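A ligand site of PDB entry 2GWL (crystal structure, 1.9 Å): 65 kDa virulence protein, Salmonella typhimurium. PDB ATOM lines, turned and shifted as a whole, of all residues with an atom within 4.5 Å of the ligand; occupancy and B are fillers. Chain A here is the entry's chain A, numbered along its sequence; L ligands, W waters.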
ATOM      1  N   ASN A  19      -9.121   6.818  -4.077  1.00  0.00           N
ATOM      2  CA  ASN A  19      -8.154   5.839  -4.593  1.00  0.00           C
ATOM      3  C   ASN A  19      -7.450   6.305  -5.861  1.00  0.00           C
ATOM      4  O   ASN A  19      -6.232   6.153  -5.975  1.00  0.00           O
ATOM      5  CB  ASN A  19      -8.792   4.442  -4.740  1.00  0.00           C
ATOM      6  CG  ASN A  19      -9.205   3.874  -3.363  1.00  0.00           C
ATOM      7  OD1 ASN A  19      -8.609   4.177  -2.365  1.00  0.00           O
ATOM      8  ND2 ASN A  19     -10.141   2.983  -3.377  1.00  0.00           N
ATOM      9  N   ARG A  23      -3.486   7.217  -6.169  1.00  0.00           N
ATOM     10  CA  ARG A  23      -2.676   6.533  -7.149  1.00  0.00           C
ATOM     11  C   ARG A  23      -1.993   7.509  -8.085  1.00  0.00           C
ATOM     12  O   ARG A  23      -1.067   7.122  -8.767  1.00  0.00           O
ATOM     13  CB  ARG A  23      -3.502   5.530  -7.960  1.00  0.00           C
ATOM     14  CG  ARG A  23      -3.893   4.310  -7.186  1.00  0.00           C
ATOM     15  CD  ARG A  23      -4.981   3.517  -7.900  1.00  0.00           C
ATOM     16  NE  ARG A  23      -5.223   2.272  -7.152  1.00  0.00           N
ATOM     17  CZ  ARG A  23      -6.390   1.666  -7.009  1.00  0.00           C
ATOM     18  NH1 ARG A  23      -7.472   2.131  -7.597  1.00  0.00           N
ATOM     19  NH2 ARG A  23      -6.460   0.539  -6.298  1.00  0.00           N
ATOM     20  N   TYR A  79      -8.196 -12.229   0.050  1.00  0.00           N
ATOM     21  CA  TYR A  79      -8.301 -12.328  -1.416  1.00  0.00           C
ATOM     22  C   TYR A  79      -8.742 -11.046  -2.044  1.00  0.00           C
ATOM     23  O   TYR A  79      -9.498 -10.251  -1.436  1.00  0.00           O
ATOM     24  CB  TYR A  79      -9.275 -13.457  -1.856  1.00  0.00           C
ATOM     25  CG  TYR A  79      -9.092 -14.664  -1.034  1.00  0.00           C
ATOM     26  CD1 TYR A  79      -8.011 -15.526  -1.273  1.00  0.00           C
ATOM     27  CD2 TYR A  79      -9.951 -14.949   0.018  1.00  0.00           C
ATOM     28  CE1 TYR A  79      -7.814 -16.676  -0.476  1.00  0.00           C
ATOM     29  CE2 TYR A  79      -9.749 -16.067   0.823  1.00  0.00           C
ATOM     30  CZ  TYR A  79      -8.685 -16.927   0.536  1.00  0.00           C
ATOM     31  OH  TYR A  79      -8.487 -18.019   1.326  1.00  0.00           O
ATOM     32  N   ARG A  80      -8.259 -10.837  -3.265  1.00  0.00           N
ATOM     33  CA  ARG A  80      -8.609  -9.664  -4.065  1.00  0.00           C
ATOM     34  C   ARG A  80      -8.601  -9.995  -5.562  1.00  0.00           C
ATOM     35  O   ARG A  80      -7.632 -10.545  -6.074  1.00  0.00           O
ATOM     36  CB  ARG A  80      -7.614  -8.574  -3.711  1.00  0.00           C
ATOM     37  CG  ARG A  80      -7.796  -7.227  -4.377  1.00  0.00           C
ATOM     38  CD  ARG A  80      -6.862  -6.243  -3.640  1.00  0.00           C
ATOM     39  NE  ARG A  80      -6.640  -4.970  -4.359  1.00  0.00           N
ATOM     40  CZ  ARG A  80      -7.551  -4.032  -4.635  1.00  0.00           C
ATOM     41  NH1 ARG A  80      -8.819  -4.147  -4.257  1.00  0.00           N
ATOM     42  NH2 ARG A  80      -7.177  -2.925  -5.299  1.00  0.00           N
ATOM     43  N   GLY A  81      -9.669  -9.663  -6.255  1.00  0.00           N
ATOM     44  CA  GLY A  81      -9.800  -9.914  -7.690  1.00  0.00           C
ATOM     45  C   GLY A  81      -9.439  -8.614  -8.347  1.00  0.00           C
ATOM     46  O   GLY A  81      -9.888  -7.505  -7.871  1.00  0.00           O
ATOM     47  N   LEU A  82      -8.649  -8.662  -9.417  1.00  0.00           N
ATOM     48  CA  LEU A  82      -8.252  -7.413 -10.146  1.00  0.00           C
ATOM     49  C   LEU A  82      -8.444  -7.679 -11.614  1.00  0.00           C
ATOM     50  O   LEU A  82      -8.249  -8.816 -12.119  1.00  0.00           O
ATOM     51  CB  LEU A  82      -6.761  -7.005  -9.928  1.00  0.00           C
ATOM     52  CG  LEU A  82      -6.166  -6.596  -8.562  1.00  0.00           C
ATOM     53  CD1 LEU A  82      -4.686  -6.225  -8.695  1.00  0.00           C
ATOM     54  CD2 LEU A  82      -6.911  -5.449  -7.884  1.00  0.00           C
ATOM     55  N   LYS A  83      -8.748  -6.633 -12.365  1.00  0.00           N
ATOM     56  CA  LYS A  83      -8.729  -6.684 -13.806  1.00  0.00           C
ATOM     57  C   LYS A  83      -7.441  -6.019 -14.219  1.00  0.00           C
ATOM     58  O   LYS A  83      -7.320  -4.787 -14.141  1.00  0.00           O
ATOM     59  CB  LYS A  83      -9.890  -5.896 -14.369  1.00  0.00           C
ATOM     60  CG  LYS A  83      -9.969  -5.911 -15.863  1.00  0.00           C
ATOM     61  CD  LYS A  83     -11.193  -5.117 -16.345  1.00  0.00           C
ATOM     62  CE  LYS A  83     -11.915  -5.809 -17.491  1.00  0.00           C
ATOM     63  NZ  LYS A  83     -13.233  -5.178 -17.758  1.00  0.00           N
ATOM     64  N   LYS A  86      -6.379  -5.021 -18.990  1.00  0.00           N
ATOM     65  CA  LYS A  86      -6.638  -3.796 -19.770  1.00  0.00           C
ATOM     66  C   LYS A  86      -5.328  -3.194 -20.321  1.00  0.00           C
ATOM     67  O   LYS A  86      -4.334  -3.106 -19.599  1.00  0.00           O
ATOM     68  CB  LYS A  86      -7.307  -2.707 -18.909  1.00  0.00           C
ATOM     69  CG  LYS A  86      -8.311  -3.168 -17.822  1.00  0.00           C
ATOM     70  CD  LYS A  86      -8.864  -1.887 -17.119  1.00  0.00           C
ATOM     71  CE  LYS A  86      -9.611  -2.169 -15.815  1.00  0.00           C
ATOM     72  NZ  LYS A  86      -9.526  -0.985 -14.841  1.00  0.00           N
ATOM     73  N   LEU A  89      -3.257  -0.772 -18.344  1.00  0.00           N
ATOM     74  CA  LEU A  89      -2.679  -1.314 -17.109  1.00  0.00           C
ATOM     75  C   LEU A  89      -1.491  -2.204 -17.401  1.00  0.00           C
ATOM     76  O   LEU A  89      -1.043  -2.975 -16.540  1.00  0.00           O
ATOM     77  CB  LEU A  89      -3.752  -2.108 -16.337  1.00  0.00           C
ATOM     78  CG  LEU A  89      -4.786  -1.204 -15.671  1.00  0.00           C
ATOM     79  CD1 LEU A  89      -5.829  -2.031 -14.964  1.00  0.00           C
ATOM     80  CD2 LEU A  89      -4.077  -0.249 -14.674  1.00  0.00           C
ATOM     81  N   VAL A  92       1.241  -1.926 -14.837  1.00  0.00           N
ATOM     82  CA  VAL A  92       0.793  -2.472 -13.573  1.00  0.00           C
ATOM     83  C   VAL A  92       0.827  -4.015 -13.648  1.00  0.00           C
ATOM     84  O   VAL A  92       1.291  -4.670 -12.727  1.00  0.00           O
ATOM     85  CB  VAL A  92      -0.615  -1.990 -13.186  1.00  0.00           C
ATOM     86  CG1 VAL A  92      -1.072  -2.642 -11.882  1.00  0.00           C
ATOM     87  CG2 VAL A  92      -0.660  -0.467 -13.037  1.00  0.00           C
ATOM     88  N   TYR A  96       3.066  -6.618 -11.259  1.00  0.00           N
ATOM     89  CA  TYR A  96       2.450  -7.699 -10.495  1.00  0.00           C
ATOM     90  C   TYR A  96       2.841  -9.077 -10.974  1.00  0.00           C
ATOM     91  O   TYR A  96       2.537 -10.040 -10.317  1.00  0.00           O
ATOM     92  CB  TYR A  96       0.916  -7.651 -10.606  1.00  0.00           C
ATOM     93  CG  TYR A  96       0.286  -6.793  -9.510  1.00  0.00           C
ATOM     94  CD1 TYR A  96       0.314  -5.407  -9.560  1.00  0.00           C
ATOM     95  CD2 TYR A  96      -0.330  -7.409  -8.426  1.00  0.00           C
ATOM     96  CE1 TYR A  96      -0.298  -4.660  -8.540  1.00  0.00           C
ATOM     97  CE2 TYR A  96      -0.948  -6.690  -7.451  1.00  0.00           C
ATOM     98  CZ  TYR A  96      -0.914  -5.317  -7.491  1.00  0.00           C
ATOM     99  OH  TYR A  96      -1.538  -4.644  -6.429  1.00  0.00           O
ATOM    100  N   ASP A 105       1.150  -0.393  -2.849  1.00  0.00           N
ATOM    101  CA  ASP A 105      -0.136   0.052  -3.301  1.00  0.00           C
ATOM    102  C   ASP A 105      -0.461   1.386  -2.625  1.00  0.00           C
ATOM    103  O   ASP A 105      -0.579   1.435  -1.401  1.00  0.00           O
ATOM    104  CB  ASP A 105      -1.200  -0.917  -2.996  1.00  0.00           C
ATOM    105  CG  ASP A 105      -2.521  -0.556  -3.724  1.00  0.00           C
ATOM    106  OD1 ASP A 105      -2.916   0.695  -3.938  1.00  0.00           O
ATOM    107  OD2 ASP A 105      -3.142  -1.474  -4.193  1.00  0.00           O
ATOM    108  N   PHE A 108      -6.094   2.943  -0.674  1.00  0.00           N
ATOM    109  CA  PHE A 108      -6.571   2.008   0.307  1.00  0.00           C
ATOM    110  C   PHE A 108      -6.788   0.686  -0.487  1.00  0.00           C
ATOM    111  O   PHE A 108      -7.216   0.733  -1.643  1.00  0.00           O
ATOM    112  CB  PHE A 108      -7.887   2.478   0.886  1.00  0.00           C
ATOM    113  CG  PHE A 108      -7.761   3.658   1.871  1.00  0.00           C
ATOM    114  CD1 PHE A 108      -7.810   3.410   3.232  1.00  0.00           C
ATOM    115  CD2 PHE A 108      -7.707   4.938   1.416  1.00  0.00           C
ATOM    116  CE1 PHE A 108      -7.727   4.461   4.145  1.00  0.00           C
ATOM    117  CE2 PHE A 108      -7.612   6.009   2.347  1.00  0.00           C
ATOM    118  CZ  PHE A 108      -7.645   5.741   3.682  1.00  0.00           C
ATOM    119  N   SER A 110      -8.737  -2.823  -0.773  1.00  0.00           N
ATOM    120  CA  SER A 110      -9.887  -3.613  -0.422  1.00  0.00           C
ATOM    121  C   SER A 110      -9.666  -5.138  -0.697  1.00  0.00           C
ATOM    122  O   SER A 110      -9.270  -5.513  -1.813  1.00  0.00           O
ATOM    123  CB  SER A 110     -11.088  -3.099  -1.199  1.00  0.00           C
ATOM    124  OG  SER A 110     -12.228  -3.743  -0.761  1.00  0.00           O
ATOM    125  N   THR A 111      -9.866  -5.959   0.309  1.00  0.00           N
ATOM    126  CA  THR A 111      -9.689  -7.389   0.188  1.00  0.00           C
ATOM    127  C   THR A 111     -10.906  -8.064   0.859  1.00  0.00           C
ATOM    128  O   THR A 111     -11.699  -7.429   1.538  1.00  0.00           O
ATOM    129  CB  THR A 111      -8.400  -7.883   0.862  1.00  0.00           C
ATOM    130  OG1 THR A 111      -8.530  -7.831   2.274  1.00  0.00           O
ATOM    131  CG2 THR A 111      -7.163  -7.157   0.452  1.00  0.00           C
ATOM    132  N   SER A 112     -11.068  -9.362   0.630  1.00  0.00           N
ATOM    133  CA  SER A 112     -12.093 -10.127   1.304  1.00  0.00           C
ATOM    134  C   SER A 112     -11.413 -11.260   2.069  1.00  0.00           C
ATOM    135  O   SER A 112     -10.534 -11.965   1.521  1.00  0.00           O
ATOM    136  CB  SER A 112     -13.066 -10.732   0.324  1.00  0.00           C
ATOM    137  OG  SER A 112     -13.815 -11.756   1.012  1.00  0.00           O
ATOM    138  N   TRP A 117     -13.472 -12.519  -5.504  1.00  0.00           N
ATOM    139  CA  TRP A 117     -14.313 -12.100  -6.579  1.00  0.00           C
ATOM    140  C   TRP A 117     -13.614 -12.371  -7.918  1.00  0.00           C
ATOM    141  O   TRP A 117     -12.490 -11.921  -8.148  1.00  0.00           O
ATOM    142  CB  TRP A 117     -14.611 -10.637  -6.346  1.00  0.00           C
ATOM    143  CG  TRP A 117     -15.526 -10.529  -5.086  1.00  0.00           C
ATOM    144  CD1 TRP A 117     -15.127 -10.374  -3.785  1.00  0.00           C
ATOM    145  CD2 TRP A 117     -16.944 -10.721  -5.062  1.00  0.00           C
ATOM    146  NE1 TRP A 117     -16.229 -10.382  -2.949  1.00  0.00           N
ATOM    147  CE2 TRP A 117     -17.359 -10.582  -3.713  1.00  0.00           C
ATOM    148  CE3 TRP A 117     -17.906 -10.910  -6.053  1.00  0.00           C
ATOM    149  CZ2 TRP A 117     -18.695 -10.659  -3.343  1.00  0.00           C
ATOM    150  CZ3 TRP A 117     -19.231 -10.973  -5.682  1.00  0.00           C
ATOM    151  CH2 TRP A 117     -19.609 -10.856  -4.334  1.00  0.00           C
ATOM    152  N   ALA A 146     -18.085  -9.695   3.712  1.00  0.00           N
ATOM    153  CA  ALA A 146     -16.947  -9.252   4.484  1.00  0.00           C
ATOM    154  C   ALA A 146     -15.869  -8.524   3.653  1.00  0.00           C
ATOM    155  O   ALA A 146     -15.653  -8.776   2.456  1.00  0.00           O
ATOM    156  CB  ALA A 146     -16.354 -10.389   5.310  1.00  0.00           C
ATOM    157  N   GLU A 147     -15.229  -7.579   4.331  1.00  0.00           N
ATOM    158  CA  GLU A 147     -14.165  -6.756   3.739  1.00  0.00           C
ATOM    159  C   GLU A 147     -13.090  -6.416   4.766  1.00  0.00           C
ATOM    160  O   GLU A 147     -13.351  -5.848   5.824  1.00  0.00           O
ATOM    161  CB  GLU A 147     -14.716  -5.463   3.115  1.00  0.00           C
ATOM    162  CG  GLU A 147     -13.633  -4.553   2.543  1.00  0.00           C
ATOM    163  CD  GLU A 147     -14.110  -3.396   1.721  1.00  0.00           C
ATOM    164  OE1 GLU A 147     -15.320  -3.196   1.594  1.00  0.00           O
ATOM    165  OE2 GLU A 147     -13.262  -2.662   1.232  1.00  0.00           O
HETATM  166  P1  LIG L   1     -10.059  -0.424  -6.429  1.00  0.00           P
HETATM  167  O1  LIG L   1      -9.341  -0.825  -5.200  1.00  0.00           O
HETATM  168  O2  LIG L   1     -10.117   1.053  -6.611  1.00  0.00           O
HETATM  169  O3  LIG L   1      -9.555  -1.327  -7.678  1.00  0.00           O
HETATM  170  C1  LIG L   1      -8.989  -0.667  -8.743  1.00  0.00           C
HETATM  171  C2  LIG L   1      -9.162  -1.352 -10.080  1.00  0.00           C
HETATM  172  O4  LIG L   1      -8.465  -0.342 -10.743  1.00  0.00           O
HETATM  173  C3  LIG L   1      -8.463  -2.687 -10.411  1.00  0.00           C
HETATM  174  O5  LIG L   1      -9.323  -3.787 -10.753  1.00  0.00           O
HETATM  175  C4  LIG L   1      -7.546  -2.320 -11.578  1.00  0.00           C
HETATM  176  O6  LIG L   1      -8.128  -2.661 -12.820  1.00  0.00           O
HETATM  177  C5  LIG L   1      -7.417  -0.785 -11.536  1.00  0.00           C
HETATM  178  N1  LIG L   1      -6.128  -0.301 -11.024  1.00  0.00           N
HETATM  179  C6  LIG L   1      -5.506   0.814 -11.520  1.00  0.00           C
HETATM  180  N2  LIG L   1      -4.319   0.973 -10.899  1.00  0.00           N
HETATM  181  C7  LIG L   1      -4.229  -0.035 -10.000  1.00  0.00           C
HETATM  182  C8  LIG L   1      -3.225  -0.302  -9.117  1.00  0.00           C
HETATM  183  N3  LIG L   1      -2.112   0.448  -9.241  1.00  0.00           N
HETATM  184  N4  LIG L   1      -3.354  -1.398  -8.296  1.00  0.00           N
HETATM  185  C9  LIG L   1      -4.458  -2.222  -8.350  1.00  0.00           C
HETATM  186  N5  LIG L   1      -5.460  -1.942  -9.237  1.00  0.00           N
HETATM  187  C10 LIG L   1      -5.338  -0.869 -10.062  1.00  0.00           C
HETATM  188  O7  LIG L   1     -11.557  -0.999  -6.328  1.00  0.00           O
HETATM  189  P2  LIG L   1     -11.996  -2.374  -5.617  1.00  0.00           P
HETATM  190  O8  LIG L   1     -11.028  -2.922  -4.601  1.00  0.00           O
HETATM  191  O9  LIG L   1     -12.411  -3.217  -6.749  1.00  0.00           O
HETATM  192  O10 LIG L   1     -13.285  -1.999  -4.737  1.00  0.00           O
HETATM  193  C11 LIG L   1     -14.537  -1.779  -5.358  1.00  0.00           C
HETATM  194  C12 LIG L   1     -15.619  -2.315  -4.424  1.00  0.00           C
HETATM  195  O11 LIG L   1     -15.414  -3.693  -4.162  1.00  0.00           O
HETATM  196  C13 LIG L   1     -15.609  -1.592  -3.075  1.00  0.00           C
HETATM  197  O12 LIG L   1     -16.924  -1.166  -2.792  1.00  0.00           O
HETATM  198  C14 LIG L   1     -15.164  -2.662  -2.096  1.00  0.00           C
HETATM  199  O13 LIG L   1     -15.936  -2.459  -0.955  1.00  0.00           O
HETATM  200  C15 LIG L   1     -15.500  -3.987  -2.796  1.00  0.00           C
HETATM  201  N6  LIG L   1     -14.564  -5.099  -2.511  1.00  0.00           N
HETATM  202  C16 LIG L   1     -13.521  -5.313  -3.388  1.00  0.00           C
HETATM  203  C17 LIG L   1     -12.611  -6.329  -3.142  1.00  0.00           C
HETATM  204  C18 LIG L   1     -11.754  -6.867  -4.299  1.00  0.00           C
HETATM  205  O14 LIG L   1     -11.464  -8.227  -4.286  1.00  0.00           O
HETATM  206  N7  LIG L   1     -11.308  -6.110  -5.332  1.00  0.00           N
HETATM  207  C19 LIG L   1     -12.796  -7.122  -1.995  1.00  0.00           C
HETATM  208  C20 LIG L   1     -13.853  -6.890  -1.116  1.00  0.00           C
HETATM  209  C21 LIG L   1     -14.757  -5.884  -1.389  1.00  0.00           C
HETATM  210  O   HOH W   1     -13.900   0.101   0.248  1.00  0.00           O
HETATM  211  O   HOH W   2     -11.869 -10.729  -3.137  1.00  0.00           O
HETATM  212  O   HOH W   3      -4.021  -3.713  -5.224  1.00  0.00           O
HETATM  213  O   HOH W   4      -1.375  -2.165  -6.638  1.00  0.00           O
HETATM  214  O   HOH W   5     -16.725  -0.713   1.425  1.00  0.00           O
HETATM  215  O   HOH W   6      -3.326   3.096 -11.974  1.00  0.00           O
HETATM  216  O   HOH W   7       0.374  -0.482  -7.323  1.00  0.00           O
HETATM  217  O   HOH W   8      -9.141  -0.698  -2.767  1.00  0.00           O
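O6 of the ligand lies within hydrogen-bond range of O of Lys 83. OE1 of Glu 147 is in hydrogen-bond range of O13 of the ligand, 2.7 Å away. An oxygen (O14) of the ligand sits at hydrogen-bond distance from the backbone NH (N) of Gly 81. O8 of the ligand is in salt-bridge range of NH1 of Arg 80. The guanidinium group (NH1) of Arg 23 lies within salt-bridge range of an oxygen (O2) of the ligand (3.0 Å). O6 of the ligand is in hydrogen-bond range of NZ of Lys 86, at 3.0 Å. A nitrogen (N6) of the ligand lies close to the side-chain hydroxyl (OG) of Ser 110 (3.2 Å). An oxygen (O5) of the ligand is in hydrogen-bond range of the backbone NH (N) of Lys 83. N7 of the ligand sits at hydrogen-bond distance from O of Gly 81, at 3.2 Å.
The guanidinium group (NH1) of Arg 80 sits at hydrogen-bond distance from the backbone carbonyl oxygen (O) of Ser 110 (2.8 Å). The backbone NH (N) of Ser 112 sits at hydrogen-bond distance from the backbone carbonyl oxygen (O) of Tyr 79, at 2.7 Å. OG of Ser 110 lies within hydrogen-bond range of OE2 of Glu 147, at 2.5 Å. The side-chain amide oxygen of Asn 19 sits at hydrogen-bond distance from the backbone NH of Phe 108, at 3.3 Å.
Asn 19 touches the ligand. Leu 82 touches the ligand (CA to O5, 3.8 Å). Leu 89 touches the ligand (CD1 to O6, 3.2 Å). Thr 111 touches the ligand (O to C20, 3.5 Å). N of Ser 112 touches C19 of the ligand (3.9 Å). The nearest printed residue that does not touch the ligand is Tyr 79 (4.01 Å).
Water W8 lies within hydrogen-bond range of an oxygen (O1) of the ligand (2.4 Å), the backbone carbonyl oxygen of Phe 108 (2.6 Å) and the backbone NH of Ser 110 (2.9 Å). Water W4 lies within hydrogen-bond range of OH of Tyr 96 (2.5 Å), N4 of the ligand (2.7 Å) and OD2 of Asp 105 (3.1 Å). Water W2 lies within hydrogen-bond range of an oxygen (O14) of the ligand (2.8 Å), the backbone carbonyl oxygen of Tyr 79 (3.0 Å) and the backbone NH of Trp 117 (3.4 Å). Water W5 lies within hydrogen-bond range of the side-chain carboxylate (OE1) of Glu 147 (2.9 Å) and an oxygen (O13) of the ligand (3.1 Å). Water W1 bridges the side-chain carboxylate (OE2) of Glu 147 and an oxygen (O13) of the ligand. Water W3 lies within hydrogen-bond range of the side-chain carboxylate (OD2) of Asp 105, the side-chain hydroxyl (OH) of Tyr 96 and the guanidinium group (NE) of Arg 80.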
